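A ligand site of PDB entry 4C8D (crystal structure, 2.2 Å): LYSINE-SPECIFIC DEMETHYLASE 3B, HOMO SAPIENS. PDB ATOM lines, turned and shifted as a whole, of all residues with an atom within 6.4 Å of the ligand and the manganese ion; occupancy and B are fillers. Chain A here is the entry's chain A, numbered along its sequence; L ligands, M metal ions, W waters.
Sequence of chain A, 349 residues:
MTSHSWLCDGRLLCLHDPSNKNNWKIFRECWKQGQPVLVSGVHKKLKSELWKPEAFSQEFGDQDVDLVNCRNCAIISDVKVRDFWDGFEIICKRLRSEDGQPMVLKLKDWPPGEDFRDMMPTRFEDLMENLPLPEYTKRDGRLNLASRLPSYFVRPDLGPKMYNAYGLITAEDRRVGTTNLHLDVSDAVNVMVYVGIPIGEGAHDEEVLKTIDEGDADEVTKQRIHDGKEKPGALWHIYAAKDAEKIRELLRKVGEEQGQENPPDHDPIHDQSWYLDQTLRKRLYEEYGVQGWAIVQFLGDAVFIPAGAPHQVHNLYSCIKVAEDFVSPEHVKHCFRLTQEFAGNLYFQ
Of the 25 residues printed, 3 come within 4 Å of the manganese ion.
The manganese ion is bound by water W1 (1.7 Å), a ring nitrogen (NE2) of His 311 (2.0 Å), an oxygen (O2) of the ligand (2.1 Å), a ring nitrogen (NE2) of His 182 (2.2 Å), the side-chain carboxylate (OD2) of Asp 184 (2.3 Å) and an oxygen (O3) of the ligand (2.3 Å).
The manganese ion has six donor atoms within binding distance.
The backbone carbonyl oxygen (O) of Asn 190 lies within hydrogen-bond range of the backbone NH (N) of Val 303 (2.8 Å).
The backbone NH (N) of Tyr 163 lies within hydrogen-bond range of the backbone carbonyl oxygen (O) of Lys 321, 2.8 Å away.
OE1 of Gln 297 lies within hydrogen-bond range of NE1 of Trp 236, 2.7 Å away.
The backbone NH (N) of Thr 179 sits at hydrogen-bond distance from the backbone carbonyl oxygen (O) of Val 313, at 2.9 Å.
A ring nitrogen (ND1) of His 182 is in hydrogen-bond range of the backbone carbonyl oxygen (O) of Asn 180, at 3.0 Å.
O of Val 313 sits at hydrogen-bond distance from N of Thr 178.
The side-chain amino group (NZ) of Lys 321 sits at hydrogen-bond distance from the side-chain amide oxygen (OD1) of Asn 315 (3.0 Å).
The backbone carbonyl oxygen (O) of Ala 188 is in hydrogen-bond range of the backbone NH (N) of Ile 305 (3.0 Å).
An oxygen (O1) of the ligand sits at hydrogen-bond distance from the side-chain amide nitrogen of Asn 190 (2.9 Å).
The side-chain amino group (NZ) of Lys 321 lies within salt-bridge range of an oxygen (O4) of the ligand, 2.6 Å away.
An oxygen (O5) of the ligand lies within hydrogen-bond range of the side-chain hydroxyl (OG1) of Thr 179, at 2.5 Å.
Water W1 lies within hydrogen-bond range of OH of Tyr 163 (3.2 Å) and OD1 of Asp 184 (3.2 Å).
Water W4 lies within hydrogen-bond range of O5 of the ligand (2.7 Å) and NZ of Lys 321 (3.4 Å).
Merely in contact with the ligand: Tyr 163 (3.5 Å), Trp 236 (3.6 Å), Ile 305 (3.6 Å) and Val 313 (3.5 Å).
Hydrophobic or aromatic side chains that line the ligand: Tyr 163, His 182, Trp 236, Ile 305, His 311 and Val 313.
Of the 25 residues printed, 10 come within 4 Å of the ligand.
Along chain A the residues within 4 Å of the ligand span positions 163 to 321.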
ATOM      1  N   LYS A 106      -3.059 -15.852  -9.753  1.00  0.00           N
ATOM      2  CA  LYS A 106      -4.335 -15.949  -9.073  1.00  0.00           C
ATOM      3  C   LYS A 106      -4.792 -14.522  -8.719  1.00  0.00           C
ATOM      4  O   LYS A 106      -3.987 -13.684  -8.314  1.00  0.00           O
ATOM      5  CB  LYS A 106      -4.182 -16.835  -7.826  1.00  0.00           C
ATOM      6  CG  LYS A 106      -5.099 -16.511  -6.658  1.00  0.00           C
ATOM      7  CD  LYS A 106      -5.198 -17.666  -5.672  1.00  0.00           C
ATOM      8  CE  LYS A 106      -3.892 -17.974  -4.978  1.00  0.00           C
ATOM      9  NZ  LYS A 106      -4.033 -19.143  -4.077  1.00  0.00           N
ATOM     10  N   TYR A 163     -13.002 -18.048  -6.799  1.00  0.00           N
ATOM     11  CA  TYR A 163     -11.627 -18.498  -6.910  1.00  0.00           C
ATOM     12  C   TYR A 163     -11.284 -18.520  -8.385  1.00  0.00           C
ATOM     13  O   TYR A 163     -11.756 -19.386  -9.142  1.00  0.00           O
ATOM     14  CB  TYR A 163     -11.446 -19.879  -6.285  1.00  0.00           C
ATOM     15  CG  TYR A 163     -11.867 -19.956  -4.845  1.00  0.00           C
ATOM     16  CD1 TYR A 163     -13.204 -20.219  -4.499  1.00  0.00           C
ATOM     17  CD2 TYR A 163     -10.948 -19.765  -3.823  1.00  0.00           C
ATOM     18  CE1 TYR A 163     -13.593 -20.278  -3.174  1.00  0.00           C
ATOM     19  CE2 TYR A 163     -11.332 -19.820  -2.491  1.00  0.00           C
ATOM     20  CZ  TYR A 163     -12.650 -20.071  -2.166  1.00  0.00           C
ATOM     21  OH  TYR A 163     -13.002 -20.153  -0.826  1.00  0.00           O
ATOM     22  N   ASN A 164     -10.486 -17.552  -8.785  1.00  0.00           N
ATOM     23  CA  ASN A 164     -10.095 -17.370 -10.158  1.00  0.00           C
ATOM     24  C   ASN A 164      -8.566 -17.440 -10.249  1.00  0.00           C
ATOM     25  O   ASN A 164      -7.881 -16.656  -9.607  1.00  0.00           O
ATOM     26  CB  ASN A 164     -10.585 -16.022 -10.656  1.00  0.00           C
ATOM     27  CG  ASN A 164     -12.060 -15.838 -10.452  1.00  0.00           C
ATOM     28  OD1 ASN A 164     -12.873 -16.670 -10.856  1.00  0.00           O
ATOM     29  ND2 ASN A 164     -12.414 -14.725  -9.834  1.00  0.00           N
ATOM     30  N   ALA A 165      -8.056 -18.397 -11.016  1.00  0.00           N
ATOM     31  CA  ALA A 165      -6.607 -18.521 -11.209  1.00  0.00           C
ATOM     32  C   ALA A 165      -6.302 -19.312 -12.459  1.00  0.00           C
ATOM     33  O   ALA A 165      -7.148 -20.072 -12.936  1.00  0.00           O
ATOM     34  CB  ALA A 165      -5.960 -19.177  -9.997  1.00  0.00           C
ATOM     35  N   THR A 178      -2.387 -24.447  -6.328  1.00  0.00           N
ATOM     36  CA  THR A 178      -3.130 -23.220  -6.645  1.00  0.00           C
ATOM     37  C   THR A 178      -3.588 -22.631  -5.303  1.00  0.00           C
ATOM     38  O   THR A 178      -3.352 -21.452  -5.015  1.00  0.00           O
ATOM     39  CB  THR A 178      -4.336 -23.527  -7.546  1.00  0.00           C
ATOM     40  OG1 THR A 178      -3.879 -24.095  -8.777  1.00  0.00           O
ATOM     41  CG2 THR A 178      -5.150 -22.271  -7.803  1.00  0.00           C
ATOM     42  N   THR A 179      -4.235 -23.469  -4.489  1.00  0.00           N
ATOM     43  CA  THR A 179      -4.570 -23.101  -3.116  1.00  0.00           C
ATOM     44  C   THR A 179      -4.039 -24.187  -2.191  1.00  0.00           C
ATOM     45  O   THR A 179      -4.366 -25.363  -2.350  1.00  0.00           O
ATOM     46  CB  THR A 179      -6.087 -22.924  -2.960  1.00  0.00           C
ATOM     47  OG1 THR A 179      -6.560 -22.058  -3.985  1.00  0.00           O
ATOM     48  CG2 THR A 179      -6.435 -22.319  -1.597  1.00  0.00           C
ATOM     49  N   ASN A 180      -3.181 -23.798  -1.258  1.00  0.00           N
ATOM     50  CA  ASN A 180      -2.587 -24.735  -0.317  1.00  0.00           C
ATOM     51  C   ASN A 180      -3.582 -25.350   0.663  1.00  0.00           C
ATOM     52  O   ASN A 180      -4.658 -24.785   0.917  1.00  0.00           O
ATOM     53  CB  ASN A 180      -1.496 -24.061   0.501  1.00  0.00           C
ATOM     54  CG  ASN A 180      -0.220 -23.882  -0.267  1.00  0.00           C
ATOM     55  OD1 ASN A 180       0.023 -24.555  -1.259  1.00  0.00           O
ATOM     56  ND2 ASN A 180       0.602 -22.960   0.199  1.00  0.00           N
ATOM     57  N   HIS A 182      -5.746 -26.280   3.557  1.00  0.00           N
ATOM     58  CA  HIS A 182      -6.336 -25.541   4.657  1.00  0.00           C
ATOM     59  C   HIS A 182      -7.720 -26.144   4.953  1.00  0.00           C
ATOM     60  O   HIS A 182      -8.135 -27.105   4.293  1.00  0.00           O
ATOM     61  CB  HIS A 182      -6.498 -24.082   4.271  1.00  0.00           C
ATOM     62  CG  HIS A 182      -7.552 -23.882   3.234  1.00  0.00           C
ATOM     63  ND1 HIS A 182      -7.438 -24.375   1.954  1.00  0.00           N
ATOM     64  CD2 HIS A 182      -8.760 -23.273   3.297  1.00  0.00           C
ATOM     65  CE1 HIS A 182      -8.518 -24.067   1.264  1.00  0.00           C
ATOM     66  NE2 HIS A 182      -9.330 -23.394   2.057  1.00  0.00           N
ATOM     67  N   LEU A 183      -8.423 -25.569   5.917  1.00  0.00           N
ATOM     68  CA  LEU A 183      -9.820 -25.922   6.141  1.00  0.00           C
ATOM     69  C   LEU A 183     -10.652 -24.657   6.230  1.00  0.00           C
ATOM     70  O   LEU A 183     -10.113 -23.597   6.485  1.00  0.00           O
ATOM     71  CB  LEU A 183      -9.975 -26.768   7.403  1.00  0.00           C
ATOM     72  CG  LEU A 183      -9.481 -26.196   8.740  1.00  0.00           C
ATOM     73  CD1 LEU A 183     -10.352 -25.058   9.244  1.00  0.00           C
ATOM     74  CD2 LEU A 183      -9.427 -27.310   9.784  1.00  0.00           C
ATOM     75  N   ASP A 184     -11.960 -24.777   6.035  1.00  0.00           N
ATOM     76  CA  ASP A 184     -12.869 -23.651   6.261  1.00  0.00           C
ATOM     77  C   ASP A 184     -13.834 -23.984   7.392  1.00  0.00           C
ATOM     78  O   ASP A 184     -14.016 -25.154   7.752  1.00  0.00           O
ATOM     79  CB  ASP A 184     -13.613 -23.261   4.962  1.00  0.00           C
ATOM     80  CG  ASP A 184     -12.688 -22.639   3.932  1.00  0.00           C
ATOM     81  OD1 ASP A 184     -12.297 -21.461   4.072  1.00  0.00           O
ATOM     82  OD2 ASP A 184     -12.333 -23.325   2.964  1.00  0.00           O
ATOM     83  N   ALA A 188     -19.469 -25.618   2.560  1.00  0.00           N
ATOM     84  CA  ALA A 188     -19.505 -24.842   1.310  1.00  0.00           C
ATOM     85  C   ALA A 188     -19.763 -25.731   0.118  1.00  0.00           C
ATOM     86  O   ALA A 188     -19.539 -26.950   0.183  1.00  0.00           O
ATOM     87  CB  ALA A 188     -18.208 -24.095   1.098  1.00  0.00           C
ATOM     88  N   VAL A 189     -20.262 -25.120  -0.954  1.00  0.00           N
ATOM     89  CA  VAL A 189     -20.306 -25.746  -2.262  1.00  0.00           C
ATOM     90  C   VAL A 189     -19.531 -24.876  -3.239  1.00  0.00           C
ATOM     91  O   VAL A 189     -19.759 -23.671  -3.334  1.00  0.00           O
ATOM     92  CB  VAL A 189     -21.756 -26.011  -2.759  1.00  0.00           C
ATOM     93  CG1 VAL A 189     -22.585 -24.731  -2.790  1.00  0.00           C
ATOM     94  CG2 VAL A 189     -21.722 -26.672  -4.128  1.00  0.00           C
ATOM     95  N   ASN A 190     -18.593 -25.494  -3.963  1.00  0.00           N
ATOM     96  CA  ASN A 190     -17.731 -24.796  -4.899  1.00  0.00           C
ATOM     97  C   ASN A 190     -18.057 -25.266  -6.292  1.00  0.00           C
ATOM     98  O   ASN A 190     -17.896 -26.439  -6.618  1.00  0.00           O
ATOM     99  CB  ASN A 190     -16.264 -25.095  -4.581  1.00  0.00           C
ATOM    100  CG  ASN A 190     -15.318 -24.474  -5.570  1.00  0.00           C
ATOM    101  OD1 ASN A 190     -15.412 -24.727  -6.780  1.00  0.00           O
ATOM    102  ND2 ASN A 190     -14.392 -23.653  -5.077  1.00  0.00           N
ATOM    103  N   ALA A 234      -9.787 -28.529 -12.258  1.00  0.00           N
ATOM    104  CA  ALA A 234      -8.886 -28.529 -11.111  1.00  0.00           C
ATOM    105  C   ALA A 234      -8.821 -29.889 -10.431  1.00  0.00           C
ATOM    106  O   ALA A 234      -9.771 -30.663 -10.500  1.00  0.00           O
ATOM    107  CB  ALA A 234      -9.303 -27.454 -10.113  1.00  0.00           C
ATOM    108  N   TRP A 236      -8.403 -31.633  -6.810  1.00  0.00           N
ATOM    109  CA  TRP A 236      -8.588 -31.426  -5.392  1.00  0.00           C
ATOM    110  C   TRP A 236      -8.097 -32.617  -4.622  1.00  0.00           C
ATOM    111  O   TRP A 236      -8.277 -33.760  -5.053  1.00  0.00           O
ATOM    112  CB  TRP A 236     -10.080 -31.321  -5.062  1.00  0.00           C
ATOM    113  CG  TRP A 236     -10.776 -30.096  -5.533  1.00  0.00           C
ATOM    114  CD1 TRP A 236     -11.050 -29.748  -6.824  1.00  0.00           C
ATOM    115  CD2 TRP A 236     -11.332 -29.066  -4.710  1.00  0.00           C
ATOM    116  NE1 TRP A 236     -11.718 -28.559  -6.858  1.00  0.00           N
ATOM    117  CE2 TRP A 236     -11.897 -28.113  -5.573  1.00  0.00           C
ATOM    118  CE3 TRP A 236     -11.397 -28.866  -3.332  1.00  0.00           C
ATOM    119  CZ2 TRP A 236     -12.540 -26.965  -5.099  1.00  0.00           C
ATOM    120  CZ3 TRP A 236     -12.023 -27.713  -2.859  1.00  0.00           C
ATOM    121  CH2 TRP A 236     -12.584 -26.781  -3.739  1.00  0.00           C
ATOM    122  N   GLN A 297     -12.263 -31.766 -10.640  1.00  0.00           N
ATOM    123  CA  GLN A 297     -13.459 -30.962 -10.823  1.00  0.00           C
ATOM    124  C   GLN A 297     -13.529 -30.479 -12.269  1.00  0.00           C
ATOM    125  O   GLN A 297     -12.732 -29.631 -12.692  1.00  0.00           O
ATOM    126  CB  GLN A 297     -13.426 -29.789  -9.847  1.00  0.00           C
ATOM    127  CG  GLN A 297     -14.669 -28.912  -9.837  1.00  0.00           C
ATOM    128  CD  GLN A 297     -14.546 -27.739  -8.882  1.00  0.00           C
ATOM    129  OE1 GLN A 297     -13.429 -27.316  -8.530  1.00  0.00           O
ATOM    130  NE2 GLN A 297     -15.695 -27.207  -8.448  1.00  0.00           N
ATOM    131  N   VAL A 303     -18.455 -29.093  -5.940  1.00  0.00           N
ATOM    132  CA  VAL A 303     -17.824 -29.854  -4.899  1.00  0.00           C
ATOM    133  C   VAL A 303     -18.329 -29.356  -3.538  1.00  0.00           C
ATOM    134  O   VAL A 303     -18.161 -28.187  -3.210  1.00  0.00           O
ATOM    135  CB  VAL A 303     -16.299 -29.697  -4.973  1.00  0.00           C
ATOM    136  CG1 VAL A 303     -15.620 -30.414  -3.815  1.00  0.00           C
ATOM    137  CG2 VAL A 303     -15.804 -30.197  -6.312  1.00  0.00           C
ATOM    138  N   ILE A 305     -17.864 -29.381   0.318  1.00  0.00           N
ATOM    139  CA  ILE A 305     -16.726 -29.512   1.214  1.00  0.00           C
ATOM    140  C   ILE A 305     -17.264 -29.343   2.618  1.00  0.00           C
ATOM    141  O   ILE A 305     -17.782 -28.265   2.950  1.00  0.00           O
ATOM    142  CB  ILE A 305     -15.695 -28.381   0.962  1.00  0.00           C
ATOM    143  CG1 ILE A 305     -15.393 -28.244  -0.539  1.00  0.00           C
ATOM    144  CG2 ILE A 305     -14.435 -28.603   1.786  1.00  0.00           C
ATOM    145  CD1 ILE A 305     -15.101 -26.817  -0.979  1.00  0.00           C
ATOM    146  N   HIS A 311      -8.511 -29.352   2.836  1.00  0.00           N
ATOM    147  CA  HIS A 311      -8.481 -29.470   1.393  1.00  0.00           C
ATOM    148  C   HIS A 311      -7.463 -28.544   0.741  1.00  0.00           C
ATOM    149  O   HIS A 311      -7.153 -27.474   1.274  1.00  0.00           O
ATOM    150  CB  HIS A 311      -9.877 -29.213   0.806  1.00  0.00           C
ATOM    151  CG  HIS A 311     -10.446 -27.866   1.137  1.00  0.00           C
ATOM    152  ND1 HIS A 311     -11.047 -27.603   2.351  1.00  0.00           N
ATOM    153  CD2 HIS A 311     -10.534 -26.727   0.414  1.00  0.00           C
ATOM    154  CE1 HIS A 311     -11.461 -26.347   2.371  1.00  0.00           C
ATOM    155  NE2 HIS A 311     -11.150 -25.794   1.214  1.00  0.00           N
ATOM    156  N   GLN A 312      -6.985 -28.994  -0.425  1.00  0.00           N
ATOM    157  CA  GLN A 312      -6.058 -28.256  -1.268  1.00  0.00           C
ATOM    158  C   GLN A 312      -6.541 -28.352  -2.718  1.00  0.00           C
ATOM    159  O   GLN A 312      -7.177 -29.337  -3.114  1.00  0.00           O
ATOM    160  CB  GLN A 312      -4.643 -28.824  -1.133  1.00  0.00           C
ATOM    161  CG  GLN A 312      -4.512 -30.292  -1.547  1.00  0.00           C
ATOM    162  CD  GLN A 312      -3.110 -30.865  -1.320  1.00  0.00           C
ATOM    163  OE1 GLN A 312      -2.367 -30.389  -0.466  1.00  0.00           O
ATOM    164  NE2 GLN A 312      -2.754 -31.896  -2.070  1.00  0.00           N
ATOM    165  N   VAL A 313      -6.197 -27.328  -3.512  1.00  0.00           N
ATOM    166  CA  VAL A 313      -6.619 -27.284  -4.913  1.00  0.00           C
ATOM    167  C   VAL A 313      -5.445 -26.967  -5.854  1.00  0.00           C
ATOM    168  O   VAL A 313      -4.564 -26.160  -5.538  1.00  0.00           O
ATOM    169  CB  VAL A 313      -7.765 -26.261  -5.112  1.00  0.00           C
ATOM    170  CG1 VAL A 313      -8.327 -26.347  -6.527  1.00  0.00           C
ATOM    171  CG2 VAL A 313      -8.858 -26.478  -4.055  1.00  0.00           C
ATOM    172  N   HIS A 314      -5.446 -27.642  -7.000  1.00  0.00           N
ATOM    173  CA  HIS A 314      -4.399 -27.512  -7.986  1.00  0.00           C
ATOM    174  C   HIS A 314      -5.075 -27.401  -9.344  1.00  0.00           C
ATOM    175  O   HIS A 314      -5.522 -28.406  -9.914  1.00  0.00           O
ATOM    176  CB  HIS A 314      -3.491 -28.750  -7.928  1.00  0.00           C
ATOM    177  CG  HIS A 314      -2.429 -28.759  -8.977  1.00  0.00           C
ATOM    178  ND1 HIS A 314      -1.113 -28.428  -8.711  1.00  0.00           N
ATOM    179  CD2 HIS A 314      -2.469 -29.051 -10.296  1.00  0.00           C
ATOM    180  CE1 HIS A 314      -0.401 -28.523  -9.817  1.00  0.00           C
ATOM    181  NE2 HIS A 314      -1.205 -28.900 -10.795  1.00  0.00           N
ATOM    182  N   ASN A 315      -5.140 -26.176  -9.849  1.00  0.00           N
ATOM    183  CA  ASN A 315      -5.745 -25.907 -11.133  1.00  0.00           C
ATOM    184  C   ASN A 315      -4.925 -26.518 -12.226  1.00  0.00           C
ATOM    185  O   ASN A 315      -3.689 -26.407 -12.220  1.00  0.00           O
ATOM    186  CB  ASN A 315      -5.878 -24.425 -11.404  1.00  0.00           C
ATOM    187  CG  ASN A 315      -6.947 -23.768 -10.557  1.00  0.00           C
ATOM    188  OD1 ASN A 315      -7.459 -24.366  -9.627  1.00  0.00           O
ATOM    189  ND2 ASN A 315      -7.294 -22.535 -10.911  1.00  0.00           N
ATOM    190  N   LYS A 321     -14.163 -20.364 -10.488  1.00  0.00           N
ATOM    191  CA  LYS A 321     -14.929 -21.076  -9.475  1.00  0.00           C
ATOM    192  C   LYS A 321     -15.681 -20.067  -8.611  1.00  0.00           C
ATOM    193  O   LYS A 321     -15.144 -19.003  -8.248  1.00  0.00           O
ATOM    194  CB  LYS A 321     -14.031 -21.925  -8.581  1.00  0.00           C
ATOM    195  CG  LYS A 321     -13.084 -22.879  -9.302  1.00  0.00           C
ATOM    196  CD  LYS A 321     -12.487 -23.868  -8.318  1.00  0.00           C
ATOM    197  CE  LYS A 321     -11.154 -24.444  -8.773  1.00  0.00           C
ATOM    198  NZ  LYS A 321     -10.044 -23.521  -8.401  1.00  0.00           N
ATOM    199  N   ALA A 323     -18.008 -20.190  -4.969  1.00  0.00           N
ATOM    200  CA  ALA A 323     -18.409 -21.002  -3.827  1.00  0.00           C
ATOM    201  C   ALA A 323     -19.454 -20.294  -2.946  1.00  0.00           C
ATOM    202  O   ALA A 323     -19.369 -19.071  -2.740  1.00  0.00           O
ATOM    203  CB  ALA A 323     -17.206 -21.372  -2.983  1.00  0.00           C
HETATM  204  C1  LIG L   1     -12.828 -23.654  -1.475  1.00  0.00           C
HETATM  205  C2  LIG L   1     -11.454 -23.533  -1.965  1.00  0.00           C
HETATM  206  C3  LIG L   1      -9.754 -23.125  -3.600  1.00  0.00           C
HETATM  207  C4  LIG L   1      -9.548 -22.934  -5.079  1.00  0.00           C
HETATM  208  O1  LIG L   1     -13.802 -23.750  -2.243  1.00  0.00           O
HETATM  209  O2  LIG L   1     -12.968 -23.650  -0.239  1.00  0.00           O
HETATM  210  O3  LIG L   1     -10.558 -23.497  -1.134  1.00  0.00           O
HETATM  211  O4  LIG L   1     -10.504 -23.168  -5.832  1.00  0.00           O
HETATM  212  N1  LIG L   1     -11.131 -23.421  -3.249  1.00  0.00           N
HETATM  213  O5  LIG L   1      -8.432 -22.540  -5.497  1.00  0.00           O
HETATM  214 MN    MN M   1     -11.268 -23.797   1.020  1.00  0.00          MN
HETATM  215  O   HOH W   1     -11.368 -22.086   1.079  1.00  0.00           O
HETATM  216  O   HOH W   2     -15.917 -23.242  -0.671  1.00  0.00           O
HETATM  217  O   HOH W   3     -15.056 -24.083   1.967  1.00  0.00           O
HETATM  218  O   HOH W   4      -8.306 -20.738  -7.469  1.00  0.00           O
